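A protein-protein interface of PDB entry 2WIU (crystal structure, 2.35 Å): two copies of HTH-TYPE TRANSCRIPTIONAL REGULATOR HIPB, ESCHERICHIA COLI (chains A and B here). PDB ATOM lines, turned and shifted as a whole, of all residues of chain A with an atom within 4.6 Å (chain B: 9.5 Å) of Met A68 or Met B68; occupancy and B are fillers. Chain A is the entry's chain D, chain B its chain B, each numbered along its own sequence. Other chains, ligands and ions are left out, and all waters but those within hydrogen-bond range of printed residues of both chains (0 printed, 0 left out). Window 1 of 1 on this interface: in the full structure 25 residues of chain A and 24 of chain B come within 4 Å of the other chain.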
ATOM      1  N   GLN A   5      13.843  10.582 -31.021  1.00  0.00           N
ATOM      2  CA  GLN A   5      13.257  11.874 -30.757  1.00  0.00           C
ATOM      3  C   GLN A   5      12.294  11.845 -29.581  1.00  0.00           C
ATOM      4  O   GLN A   5      12.313  12.729 -28.767  1.00  0.00           O
ATOM      5  CB  GLN A   5      12.592  12.454 -31.999  1.00  0.00           C
ATOM      6  CG  GLN A   5      13.125  13.823 -32.353  1.00  0.00           C
ATOM      7  CD  GLN A   5      12.172  14.694 -33.165  1.00  0.00           C
ATOM      8  OE1 GLN A   5      12.560  15.268 -34.176  1.00  0.00           O
ATOM      9  NE2 GLN A   5      10.942  14.818 -32.710  1.00  0.00           N
ATOM     10  N   LYS A   6      11.470  10.822 -29.485  1.00  0.00           N
ATOM     11  CA  LYS A   6      10.527  10.711 -28.395  1.00  0.00           C
ATOM     12  C   LYS A   6      11.127  10.065 -27.199  1.00  0.00           C
ATOM     13  O   LYS A   6      11.853   9.136 -27.320  1.00  0.00           O
ATOM     14  CB  LYS A   6       9.333   9.929 -28.827  1.00  0.00           C
ATOM     15  CG  LYS A   6       8.356  10.733 -29.528  1.00  0.00           C
ATOM     16  CD  LYS A   6       7.324   9.865 -30.095  1.00  0.00           C
ATOM     17  CE  LYS A   6       6.503  10.564 -31.086  1.00  0.00           C
ATOM     18  NZ  LYS A   6       5.206   9.912 -31.160  1.00  0.00           N
ATOM     19  N   ILE A   7      10.815  10.567 -26.034  1.00  0.00           N
ATOM     20  CA  ILE A   7      11.551  10.146 -24.868  1.00  0.00           C
ATOM     21  C   ILE A   7      10.602   9.719 -23.754  1.00  0.00           C
ATOM     22  O   ILE A   7       9.553  10.368 -23.606  1.00  0.00           O
ATOM     23  CB  ILE A   7      12.385  11.345 -24.356  1.00  0.00           C
ATOM     24  CG1 ILE A   7      13.528  11.708 -25.327  1.00  0.00           C
ATOM     25  CG2 ILE A   7      12.963  11.126 -22.966  1.00  0.00           C
ATOM     26  CD1 ILE A   7      14.436  12.703 -24.698  1.00  0.00           C
ATOM     27  N   LEU A  13      16.425  10.563 -21.021  1.00  0.00           N
ATOM     28  CA  LEU A  13      16.395  12.001 -21.068  1.00  0.00           C
ATOM     29  C   LEU A  13      17.750  12.524 -20.603  1.00  0.00           C
ATOM     30  O   LEU A  13      18.409  13.254 -21.330  1.00  0.00           O
ATOM     31  CB  LEU A  13      15.318  12.491 -20.086  1.00  0.00           C
ATOM     32  CG  LEU A  13      15.226  14.006 -19.874  1.00  0.00           C
ATOM     33  CD1 LEU A  13      14.792  14.684 -21.181  1.00  0.00           C
ATOM     34  CD2 LEU A  13      14.205  14.305 -18.786  1.00  0.00           C
ATOM     35  N   PHE A  57      15.751  19.938 -13.167  1.00  0.00           N
ATOM     36  CA  PHE A  57      15.716  19.582 -14.574  1.00  0.00           C
ATOM     37  C   PHE A  57      15.534  20.783 -15.511  1.00  0.00           C
ATOM     38  O   PHE A  57      16.143  20.844 -16.580  1.00  0.00           O
ATOM     39  CB  PHE A  57      14.623  18.532 -14.852  1.00  0.00           C
ATOM     40  CG  PHE A  57      14.231  18.453 -16.316  1.00  0.00           C
ATOM     41  CD1 PHE A  57      15.101  17.968 -17.250  1.00  0.00           C
ATOM     42  CD2 PHE A  57      13.000  18.882 -16.742  1.00  0.00           C
ATOM     43  CE1 PHE A  57      14.761  17.884 -18.598  1.00  0.00           C
ATOM     44  CE2 PHE A  57      12.643  18.824 -18.079  1.00  0.00           C
ATOM     45  CZ  PHE A  57      13.515  18.341 -19.007  1.00  0.00           C
ATOM     46  N   PHE A  58      14.659  21.718 -15.172  1.00  0.00           N
ATOM     47  CA  PHE A  58      14.409  22.842 -16.090  1.00  0.00           C
ATOM     48  C   PHE A  58      15.571  23.871 -16.031  1.00  0.00           C
ATOM     49  O   PHE A  58      15.962  24.436 -17.051  1.00  0.00           O
ATOM     50  CB  PHE A  58      13.014  23.476 -15.866  1.00  0.00           C
ATOM     51  CG  PHE A  58      11.903  22.794 -16.616  1.00  0.00           C
ATOM     52  CD1 PHE A  58      11.766  22.962 -17.962  1.00  0.00           C
ATOM     53  CD2 PHE A  58      11.015  21.962 -15.972  1.00  0.00           C
ATOM     54  CE1 PHE A  58      10.778  22.327 -18.666  1.00  0.00           C
ATOM     55  CE2 PHE A  58      10.022  21.319 -16.672  1.00  0.00           C
ATOM     56  CZ  PHE A  58       9.894  21.518 -18.022  1.00  0.00           C
ATOM     57  N   LEU A  61      18.124  22.348 -18.127  1.00  0.00           N
ATOM     58  CA  LEU A  61      17.649  22.398 -19.507  1.00  0.00           C
ATOM     59  C   LEU A  61      17.857  23.790 -20.111  1.00  0.00           C
ATOM     60  O   LEU A  61      18.171  23.913 -21.286  1.00  0.00           O
ATOM     61  CB  LEU A  61      16.143  22.070 -19.516  1.00  0.00           C
ATOM     62  CG  LEU A  61      15.441  21.863 -20.859  1.00  0.00           C
ATOM     63  CD1 LEU A  61      15.889  20.515 -21.525  1.00  0.00           C
ATOM     64  CD2 LEU A  61      13.960  21.843 -20.561  1.00  0.00           C
ATOM     65  N   SER A  67      14.564  23.718 -24.920  1.00  0.00           N
ATOM     66  CA  SER A  67      13.307  23.485 -24.225  1.00  0.00           C
ATOM     67  C   SER A  67      12.849  22.043 -24.473  1.00  0.00           C
ATOM     68  O   SER A  67      13.568  21.228 -25.071  1.00  0.00           O
ATOM     69  CB  SER A  67      12.243  24.464 -24.740  1.00  0.00           C
ATOM     70  OG  SER A  67      12.265  24.250 -26.135  1.00  0.00           O
ATOM     71  N   MET A  68      11.635  21.751 -24.005  1.00  0.00           N
ATOM     72  CA  MET A  68      11.027  20.469 -24.215  1.00  0.00           C
ATOM     73  C   MET A  68       9.601  20.697 -24.688  1.00  0.00           C
ATOM     74  O   MET A  68       9.000  21.704 -24.376  1.00  0.00           O
ATOM     75  CB  MET A  68      11.029  19.701 -22.895  1.00  0.00           C
ATOM     76  CG  MET A  68      10.112  20.329 -21.896  1.00  0.00           C
ATOM     77  SD  MET A  68       9.371  19.138 -20.788  1.00  0.00           S
ATOM     78  CE  MET A  68       8.287  18.257 -21.841  1.00  0.00           C
ATOM     79  N   THR A  69       9.066  19.746 -25.449  1.00  0.00           N
ATOM     80  CA  THR A  69       7.664  19.738 -25.833  1.00  0.00           C
ATOM     81  C   THR A  69       7.019  18.392 -25.470  1.00  0.00           C
ATOM     82  O   THR A  69       7.720  17.416 -25.185  1.00  0.00           O
ATOM     83  CB  THR A  69       7.550  20.085 -27.330  1.00  0.00           C
ATOM     84  OG1 THR A  69       6.231  20.566 -27.639  1.00  0.00           O
ATOM     85  CG2 THR A  69       7.920  18.890 -28.220  1.00  0.00           C
ATOM     86  N   LEU A  70       5.689  18.340 -25.468  1.00  0.00           N
ATOM     87  CA  LEU A  70       4.922  17.113 -25.249  1.00  0.00           C
ATOM     88  C   LEU A  70       4.452  16.595 -26.595  1.00  0.00           C
ATOM     89  O   LEU A  70       4.105  17.400 -27.442  1.00  0.00           O
ATOM     90  CB  LEU A  70       3.693  17.463 -24.435  1.00  0.00           C
ATOM     91  CG  LEU A  70       3.882  17.899 -22.987  1.00  0.00           C
ATOM     92  CD1 LEU A  70       2.576  18.433 -22.408  1.00  0.00           C
ATOM     93  CD2 LEU A  70       4.434  16.808 -22.118  1.00  0.00           C
ATOM     94  N   CYS A  71       4.461  15.280 -26.816  1.00  0.00           N
ATOM     95  CA  CYS A  71       3.982  14.654 -28.056  1.00  0.00           C
ATOM     96  C   CYS A  71       2.846  13.680 -27.768  1.00  0.00           C
ATOM     97  O   CYS A  71       2.783  13.098 -26.707  1.00  0.00           O
ATOM     98  CB  CYS A  71       5.100  13.842 -28.769  1.00  0.00           C
ATOM     99  SG  CYS A  71       6.845  14.437 -28.586  1.00  0.00           S
ATOM    100  N   LYS B   6       6.494  24.654 -26.844  1.00  0.00           N
ATOM    101  CA  LYS B   6       7.750  24.891 -26.028  1.00  0.00           C
ATOM    102  C   LYS B   6       7.667  25.314 -24.564  1.00  0.00           C
ATOM    103  O   LYS B   6       7.021  26.304 -24.235  1.00  0.00           O
ATOM    104  CB  LYS B   6       8.765  25.775 -26.721  1.00  0.00           C
ATOM    105  CG  LYS B   6       9.563  25.136 -27.814  1.00  0.00           C
ATOM    106  CD  LYS B   6      10.476  26.209 -28.454  1.00  0.00           C
ATOM    107  CE  LYS B   6      10.622  25.991 -29.950  1.00  0.00           C
ATOM    108  NZ  LYS B   6      12.045  26.213 -30.389  1.00  0.00           N
ATOM    109  N   ILE B   7       8.321  24.551 -23.683  1.00  0.00           N
ATOM    110  CA  ILE B   7       7.961  24.529 -22.278  1.00  0.00           C
ATOM    111  C   ILE B   7       9.242  24.690 -21.444  1.00  0.00           C
ATOM    112  O   ILE B   7      10.268  24.127 -21.791  1.00  0.00           O
ATOM    113  CB  ILE B   7       7.250  23.205 -21.905  1.00  0.00           C
ATOM    114  CG1 ILE B   7       5.846  23.115 -22.491  1.00  0.00           C
ATOM    115  CG2 ILE B   7       7.081  23.032 -20.401  1.00  0.00           C
ATOM    116  CD1 ILE B   7       5.358  21.655 -22.609  1.00  0.00           C
ATOM    117  N   TYR B   8       9.181  25.455 -20.351  1.00  0.00           N
ATOM    118  CA  TYR B   8      10.399  26.025 -19.784  1.00  0.00           C
ATOM    119  C   TYR B   8      10.379  26.053 -18.278  1.00  0.00           C
ATOM    120  O   TYR B   8      11.395  26.447 -17.682  1.00  0.00           O
ATOM    121  CB  TYR B   8      10.611  27.487 -20.249  1.00  0.00           C
ATOM    122  CG  TYR B   8      10.970  27.686 -21.700  1.00  0.00           C
ATOM    123  CD1 TYR B   8      12.277  27.589 -22.154  1.00  0.00           C
ATOM    124  CD2 TYR B   8       9.994  27.969 -22.622  1.00  0.00           C
ATOM    125  CE1 TYR B   8      12.585  27.801 -23.501  1.00  0.00           C
ATOM    126  CE2 TYR B   8      10.296  28.164 -23.964  1.00  0.00           C
ATOM    127  CZ  TYR B   8      11.593  28.094 -24.383  1.00  0.00           C
ATOM    128  OH  TYR B   8      11.828  28.302 -25.732  1.00  0.00           O
ATOM    129  N   SER B   9       9.235  25.718 -17.668  1.00  0.00           N
ATOM    130  CA  SER B   9       9.209  25.509 -16.215  1.00  0.00           C
ATOM    131  C   SER B   9       8.328  24.329 -15.761  1.00  0.00           C
ATOM    132  O   SER B   9       7.423  23.911 -16.459  1.00  0.00           O
ATOM    133  CB  SER B   9       8.719  26.790 -15.498  1.00  0.00           C
ATOM    134  OG  SER B   9       7.456  27.154 -16.033  1.00  0.00           O
ATOM    135  N   PRO B  10       8.556  23.817 -14.549  1.00  0.00           N
ATOM    136  CA  PRO B  10       7.593  22.851 -14.037  1.00  0.00           C
ATOM    137  C   PRO B  10       6.132  23.325 -14.075  1.00  0.00           C
ATOM    138  O   PRO B  10       5.245  22.576 -14.474  1.00  0.00           O
ATOM    139  CB  PRO B  10       8.057  22.615 -12.597  1.00  0.00           C
ATOM    140  CG  PRO B  10       9.492  23.073 -12.548  1.00  0.00           C
ATOM    141  CD  PRO B  10       9.679  24.080 -13.627  1.00  0.00           C
ATOM    142  N   GLN B  12       4.608  25.432 -16.185  1.00  0.00           N
ATOM    143  CA  GLN B  12       4.010  25.456 -17.513  1.00  0.00           C
ATOM    144  C   GLN B  12       3.746  24.025 -17.999  1.00  0.00           C
ATOM    145  O   GLN B  12       2.885  23.800 -18.854  1.00  0.00           O
ATOM    146  CB  GLN B  12       4.999  26.121 -18.473  1.00  0.00           C
ATOM    147  CG  GLN B  12       4.464  26.413 -19.860  1.00  0.00           C
ATOM    148  CD  GLN B  12       5.546  26.759 -20.819  1.00  0.00           C
ATOM    149  OE1 GLN B  12       6.681  27.078 -20.417  1.00  0.00           O
ATOM    150  NE2 GLN B  12       5.227  26.684 -22.099  1.00  0.00           N
ATOM    151  N   LEU B  13       4.550  23.088 -17.485  1.00  0.00           N
ATOM    152  CA  LEU B  13       4.447  21.692 -17.816  1.00  0.00           C
ATOM    153  C   LEU B  13       3.194  21.037 -17.194  1.00  0.00           C
ATOM    154  O   LEU B  13       2.411  20.414 -17.886  1.00  0.00           O
ATOM    155  CB  LEU B  13       5.682  20.979 -17.311  1.00  0.00           C
ATOM    156  CG  LEU B  13       5.699  19.485 -17.616  1.00  0.00           C
ATOM    157  CD1 LEU B  13       5.673  19.318 -19.127  1.00  0.00           C
ATOM    158  CD2 LEU B  13       6.997  18.947 -17.005  1.00  0.00           C
ATOM    159  N   ALA B  14       3.039  21.194 -15.888  1.00  0.00           N
ATOM    160  CA  ALA B  14       1.898  20.784 -15.130  1.00  0.00           C
ATOM    161  C   ALA B  14       0.605  21.345 -15.711  1.00  0.00           C
ATOM    162  O   ALA B  14      -0.381  20.630 -15.869  1.00  0.00           O
ATOM    163  CB  ALA B  14       2.087  21.211 -13.699  1.00  0.00           C
ATOM    164  N   ALA B  16       0.020  22.139 -18.820  1.00  0.00           N
ATOM    165  CA  ALA B  16      -0.348  21.643 -20.133  1.00  0.00           C
ATOM    166  C   ALA B  16      -0.833  20.185 -19.946  1.00  0.00           C
ATOM    167  O   ALA B  16      -1.617  19.696 -20.749  1.00  0.00           O
ATOM    168  CB  ALA B  16       0.836  21.703 -21.088  1.00  0.00           C
ATOM    169  N   MET B  17      -0.337  19.539 -18.915  1.00  0.00           N
ATOM    170  CA  MET B  17      -0.624  18.163 -18.644  1.00  0.00           C
ATOM    171  C   MET B  17      -1.959  18.024 -17.962  1.00  0.00           C
ATOM    172  O   MET B  17      -2.707  17.152 -18.258  1.00  0.00           O
ATOM    173  CB  MET B  17       0.493  17.519 -17.841  1.00  0.00           C
ATOM    174  CG  MET B  17       1.549  16.922 -18.714  1.00  0.00           C
ATOM    175  SD  MET B  17       3.096  16.518 -17.981  1.00  0.00           S
ATOM    176  CE  MET B  17       2.793  14.938 -17.351  1.00  0.00           C
ATOM    177  N   PHE B  45       1.433  17.192  -8.084  1.00  0.00           N
ATOM    178  CA  PHE B  45       2.156  17.556  -9.282  1.00  0.00           C
ATOM    179  C   PHE B  45       1.397  18.709  -9.980  1.00  0.00           C
ATOM    180  O   PHE B  45       2.006  19.618 -10.517  1.00  0.00           O
ATOM    181  CB  PHE B  45       2.293  16.330 -10.200  1.00  0.00           C
ATOM    182  CG  PHE B  45       2.515  16.684 -11.641  1.00  0.00           C
ATOM    183  CD1 PHE B  45       3.733  17.160 -12.075  1.00  0.00           C
ATOM    184  CD2 PHE B  45       1.490  16.542 -12.558  1.00  0.00           C
ATOM    185  CE1 PHE B  45       3.937  17.491 -13.398  1.00  0.00           C
ATOM    186  CE2 PHE B  45       1.663  16.865 -13.885  1.00  0.00           C
ATOM    187  CZ  PHE B  45       2.910  17.365 -14.309  1.00  0.00           C
ATOM    188  N   LEU B  54      11.623  13.231 -11.506  1.00  0.00           N
ATOM    189  CA  LEU B  54      11.477  12.874 -12.888  1.00  0.00           C
ATOM    190  C   LEU B  54      10.770  11.556 -13.106  1.00  0.00           C
ATOM    191  O   LEU B  54      10.100  11.364 -14.075  1.00  0.00           O
ATOM    192  CB  LEU B  54      12.828  12.873 -13.561  1.00  0.00           C
ATOM    193  CG  LEU B  54      13.391  14.216 -13.984  1.00  0.00           C
ATOM    194  CD1 LEU B  54      14.706  14.039 -14.584  1.00  0.00           C
ATOM    195  CD2 LEU B  54      12.504  14.914 -14.909  1.00  0.00           C
ATOM    196  N   PHE B  57       6.897  12.127 -12.862  1.00  0.00           N
ATOM    197  CA  PHE B  57       6.506  12.874 -14.037  1.00  0.00           C
ATOM    198  C   PHE B  57       6.311  11.930 -15.204  1.00  0.00           C
ATOM    199  O   PHE B  57       5.303  12.017 -15.929  1.00  0.00           O
ATOM    200  CB  PHE B  57       7.595  13.935 -14.396  1.00  0.00           C
ATOM    201  CG  PHE B  57       7.601  14.333 -15.865  1.00  0.00           C
ATOM    202  CD1 PHE B  57       6.566  15.085 -16.400  1.00  0.00           C
ATOM    203  CD2 PHE B  57       8.622  13.935 -16.698  1.00  0.00           C
ATOM    204  CE1 PHE B  57       6.551  15.463 -17.761  1.00  0.00           C
ATOM    205  CE2 PHE B  57       8.642  14.294 -18.040  1.00  0.00           C
ATOM    206  CZ  PHE B  57       7.603  15.058 -18.579  1.00  0.00           C
ATOM    207  N   PHE B  58       7.305  11.076 -15.453  1.00  0.00           N
ATOM    208  CA  PHE B  58       7.188  10.141 -16.576  1.00  0.00           C
ATOM    209  C   PHE B  58       6.071   9.080 -16.417  1.00  0.00           C
ATOM    210  O   PHE B  58       5.502   8.594 -17.411  1.00  0.00           O
ATOM    211  CB  PHE B  58       8.563   9.522 -16.827  1.00  0.00           C
ATOM    212  CG  PHE B  58       9.399  10.336 -17.761  1.00  0.00           C
ATOM    213  CD1 PHE B  58       9.064  10.413 -19.100  1.00  0.00           C
ATOM    214  CD2 PHE B  58      10.490  11.056 -17.295  1.00  0.00           C
ATOM    215  CE1 PHE B  58       9.820  11.181 -19.984  1.00  0.00           C
ATOM    216  CE2 PHE B  58      11.263  11.802 -18.170  1.00  0.00           C
ATOM    217  CZ  PHE B  58      10.919  11.873 -19.508  1.00  0.00           C
ATOM    218  N   LEU B  61       3.062  11.001 -17.340  1.00  0.00           N
ATOM    219  CA  LEU B  61       3.123  11.171 -18.791  1.00  0.00           C
ATOM    220  C   LEU B  61       2.726   9.906 -19.586  1.00  0.00           C
ATOM    221  O   LEU B  61       2.107   9.951 -20.665  1.00  0.00           O
ATOM    222  CB  LEU B  61       4.558  11.630 -19.097  1.00  0.00           C
ATOM    223  CG  LEU B  61       4.976  12.073 -20.485  1.00  0.00           C
ATOM    224  CD1 LEU B  61       4.466  13.505 -20.722  1.00  0.00           C
ATOM    225  CD2 LEU B  61       6.487  11.996 -20.614  1.00  0.00           C
ATOM    226  N   GLN B  62       3.106   8.746 -19.067  1.00  0.00           N
ATOM    227  CA  GLN B  62       2.784   7.495 -19.764  1.00  0.00           C
ATOM    228  C   GLN B  62       1.265   7.281 -19.690  1.00  0.00           C
ATOM    229  O   GLN B  62       0.597   6.953 -20.677  1.00  0.00           O
ATOM    230  CB  GLN B  62       3.557   6.323 -19.130  1.00  0.00           C
ATOM    231  CG  GLN B  62       5.059   6.302 -19.432  1.00  0.00           C
ATOM    232  CD  GLN B  62       5.345   5.731 -20.799  1.00  0.00           C
ATOM    233  OE1 GLN B  62       4.579   5.903 -21.764  1.00  0.00           O
ATOM    234  NE2 GLN B  62       6.458   5.034 -20.894  1.00  0.00           N
ATOM    235  N   GLU B  65      -0.730   9.148 -21.992  1.00  0.00           N
ATOM    236  CA  GLU B  65      -0.552   8.731 -23.355  1.00  0.00           C
ATOM    237  C   GLU B  65       0.290   9.694 -24.164  1.00  0.00           C
ATOM    238  O   GLU B  65       0.076   9.875 -25.323  1.00  0.00           O
ATOM    239  CB  GLU B  65      -1.899   8.578 -23.996  1.00  0.00           C
ATOM    240  CG  GLU B  65      -2.215   7.214 -24.442  1.00  0.00           C
ATOM    241  CD  GLU B  65      -3.511   6.718 -23.927  1.00  0.00           C
ATOM    242  OE1 GLU B  65      -4.542   7.044 -24.494  1.00  0.00           O
ATOM    243  OE2 GLU B  65      -3.503   5.971 -22.960  1.00  0.00           O
ATOM    244  N   LEU B  66       1.261  10.296 -23.510  1.00  0.00           N
ATOM    245  CA  LEU B  66       2.138  11.278 -24.101  1.00  0.00           C
ATOM    246  C   LEU B  66       3.575  10.818 -24.000  1.00  0.00           C
ATOM    247  O   LEU B  66       3.889  10.020 -23.177  1.00  0.00           O
ATOM    248  CB  LEU B  66       1.996  12.588 -23.333  1.00  0.00           C
ATOM    249  CG  LEU B  66       0.684  13.343 -23.321  1.00  0.00           C
ATOM    250  CD1 LEU B  66       0.665  14.432 -22.346  1.00  0.00           C
ATOM    251  CD2 LEU B  66       0.296  13.857 -24.628  1.00  0.00           C
ATOM    252  N   SER B  67       4.449  11.344 -24.841  1.00  0.00           N
ATOM    253  CA  SER B  67       5.876  11.353 -24.552  1.00  0.00           C
ATOM    254  C   SER B  67       6.235  12.834 -24.654  1.00  0.00           C
ATOM    255  O   SER B  67       5.362  13.681 -24.709  1.00  0.00           O
ATOM    256  CB  SER B  67       6.662  10.571 -25.611  1.00  0.00           C
ATOM    257  OG  SER B  67       6.281  11.032 -26.910  1.00  0.00           O
ATOM    258  N   MET B  68       7.519  13.100 -24.657  1.00  0.00           N
ATOM    259  CA  MET B  68       8.059  14.409 -24.627  1.00  0.00           C
ATOM    260  C   MET B  68       9.223  14.407 -25.561  1.00  0.00           C
ATOM    261  O   MET B  68       9.742  13.383 -25.882  1.00  0.00           O
ATOM    262  CB  MET B  68       8.585  14.681 -23.248  1.00  0.00           C
ATOM    263  CG  MET B  68      10.023  14.329 -23.159  1.00  0.00           C
ATOM    264  SD  MET B  68      10.711  14.705 -21.636  1.00  0.00           S
ATOM    265  CE  MET B  68      11.595  16.124 -22.061  1.00  0.00           C
ATOM    266  N   THR B  69       9.646  15.573 -25.986  1.00  0.00           N
ATOM    267  CA  THR B  69      10.864  15.675 -26.736  1.00  0.00           C
ATOM    268  C   THR B  69      11.688  16.867 -26.283  1.00  0.00           C
ATOM    269  O   THR B  69      11.250  17.632 -25.473  1.00  0.00           O
ATOM    270  CB  THR B  69      10.600  15.664 -28.213  1.00  0.00           C
ATOM    271  OG1 THR B  69      11.816  15.418 -28.876  1.00  0.00           O
ATOM    272  CG2 THR B  69      10.086  16.930 -28.664  1.00  0.00           C
ATOM    273  N   LEU B  70      12.911  16.978 -26.760  1.00  0.00           N
ATOM    274  CA  LEU B  70      13.759  18.119 -26.470  1.00  0.00           C
ATOM    275  C   LEU B  70      13.817  19.045 -27.654  1.00  0.00           C
ATOM    276  O   LEU B  70      13.801  18.598 -28.767  1.00  0.00           O
ATOM    277  CB  LEU B  70      15.156  17.662 -26.114  1.00  0.00           C
ATOM    278  CG  LEU B  70      15.269  16.818 -24.867  1.00  0.00           C
ATOM    279  CD1 LEU B  70      16.562  16.153 -24.784  1.00  0.00           C
ATOM    280  CD2 LEU B  70      15.035  17.599 -23.675  1.00  0.00           C
ATOM    281  N   CYS B  71      13.872  20.343 -27.405  1.00  0.00           N
ATOM    282  CA  CYS B  71      13.941  21.308 -28.526  1.00  0.00           C
ATOM    283  C   CYS B  71      15.137  22.242 -28.375  1.00  0.00           C
ATOM    284  O   CYS B  71      15.600  22.467 -27.257  1.00  0.00           O
ATOM    285  CB  CYS B  71      12.665  22.177 -28.622  1.00  0.00           C
ATOM    286  SG  CYS B  71      11.051  21.395 -28.145  1.00  0.00           S
ATOM    287  N   ASP B  72      15.602  22.801 -29.488  1.00  0.00           N
ATOM    288  CA  ASP B  72      16.106  24.193 -29.548  1.00  0.00           C
ATOM    289  C   ASP B  72      15.048  25.292 -29.551  1.00  0.00           C
ATOM    290  O   ASP B  72      14.646  25.780 -28.485  1.00  0.00           O
ATOM    291  CB  ASP B  72      17.064  24.370 -30.726  1.00  0.00           C
ATOM    292  CG  ASP B  72      18.152  23.303 -30.733  1.00  0.00           C
ATOM    293  OD1 ASP B  72      18.891  23.183 -29.735  1.00  0.00           O
ATOM    294  OD2 ASP B  72      18.263  22.554 -31.720  1.00  0.00           O
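Printed residues of chain A that touch a printed residue of chain B: Gln A5, Lys A6, Ile A7, Leu A13, Phe A58, Leu A61, Ser A67, Met A68, Thr A69, Leu A70 and Cys A71. Hydrophobic or aromatic side chains of chain A that line the printed part of chain B: Ile A7, Leu A13, Phe A58, Leu A61, Met A68 and Leu A70. Hydrophobic or aromatic side chains of chain B within 4 Å of the printed part of chain A: Ile B7, Tyr B8, Pro B10, Leu B13, Ala B16, Phe B58, Leu B61, Leu B66, Met B68 and Leu B70. Among the printed residues, 38 pairs touch across the chains. Among the printed residues, no Asp or Glu carboxylate lies within 4 Å of a Lys or Arg side-chain nitrogen of the other chain.
Among the printed residues, merely in contact across the chains: Gln A5 with Met B68, Lys A6 with Ser B67, Lys A6 with Met B68, Ile A7 with Phe B58, Ile A7 with Ser B67, Leu A13 with Phe B58, Leu A13 with Met B68, Leu A13 with Leu B70, Phe A58 with Ile B7, Phe A58 with Tyr B8, Phe A58 with Ser B9, Phe A58 with Pro B10, Phe A58 with Leu B13, Leu A61 with Leu B70, Ser A67 with Lys B6, Ser A67 with Ile B7, Ser A67 with Tyr B8, Ser A67 with Leu B70, Ser A67 with Asp B72, Met A68 with Lys B6, Met A68 with Leu B13, Met A68 with Met B68, Met A68 with Thr B69, Met A68 with Cys B71, Thr A69 with Met B68, Leu A70 with Ala B16, Leu A70 with Leu B61, Leu A70 with Ser B67, Cys A71 with Leu B66, Cys A71 with Met B68 and Cys A71 with Thr B69.
Met A68 touches just these residues of chain B: Lys B6, Ile B7, Leu B13, Met B68, Thr B69 and Cys B71. Met B68 touches just these residues of chain A: Gln A5 (3.9 Å), Lys A6 (3.8 Å), Ile A7 (3.0 Å), Leu A13 (3.6 Å), Met A68 (3.7 Å), Thr A69 (3.1 Å) and Cys A71 (3.8 Å). Of chain B, only Lys B6, Ile B7, Tyr B8, Leu B70, Cys B71 and Asp B72 come within 4 Å of Ser A67. Of chain B, only Met B68 (3.1 Å), Thr B69 (2.8 Å) and Cys B71 (3.7 Å) come within 4 Å of Thr A69. Of the printed residues of chain A, Thr B69 touches Gln A5, Met A68, Thr A69 and Cys A71. Of the printed residues of chain B, Leu A61 touches Leu B70. Printed residues of chain A within 4 Å of Phe B58: Ile A7 and Leu A13.
Leu A13 touches Leu B70, but with the chains exchanged Leu A70 does not touch Leu B13 (4.1 Å). Ser A67 touches Cys B71, and with the chains exchanged Cys A71 touches Ser B67. Met A68 touches Cys B71, and with the chains exchanged Cys A71 touches Met B68. Thr A69 touches its own counterpart, Thr B69. 11 positions are printed for both chains. Of the 38 pairs that touch across the chains among the printed residues, 28 have their exchanged pair printed and touching as well.
The backbone carbonyl oxygen of Met B68 lies within hydrogen-bond range of the backbone NH of Ile A7 (3.0 Å). N of Thr A69 sits close to SG of Cys B71, at 3.7 Å. The backbone NH of Thr B69 lies within hydrogen-bond range of the backbone carbonyl oxygen of Thr A69, 2.8 Å away. O of Ser B67 sits at hydrogen-bond distance from N of Cys A71 (2.8 Å). The backbone carbonyl oxygen (O) of Met A68 is in hydrogen-bond range of the backbone NH (N) of Ile B7. The side-chain hydroxyl (OG1) of Thr B69 lies within hydrogen-bond range of the backbone carbonyl oxygen (O) of Gln A5 (2.7 Å). O of Ser A67 is in hydrogen-bond range of N of Cys B71 (2.5 Å).
O of Asp B72 lies close to NZ of Lys B6, 3.3 Å away. OE1 of Gln B12 sits at hydrogen-bond distance from N of Tyr B8, at 3.0 Å. The backbone carbonyl oxygen (O) of Lys B6 sits at hydrogen-bond distance from the side-chain amide nitrogen (NE2) of Gln B12. The side-chain hydroxyl (OG) of Ser B9 is in hydrogen-bond range of the backbone NH (N) of Gln B12. The backbone carbonyl oxygen (O) of Leu B61 sits at hydrogen-bond distance from the backbone NH (N) of Leu B66, 3.0 Å away.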
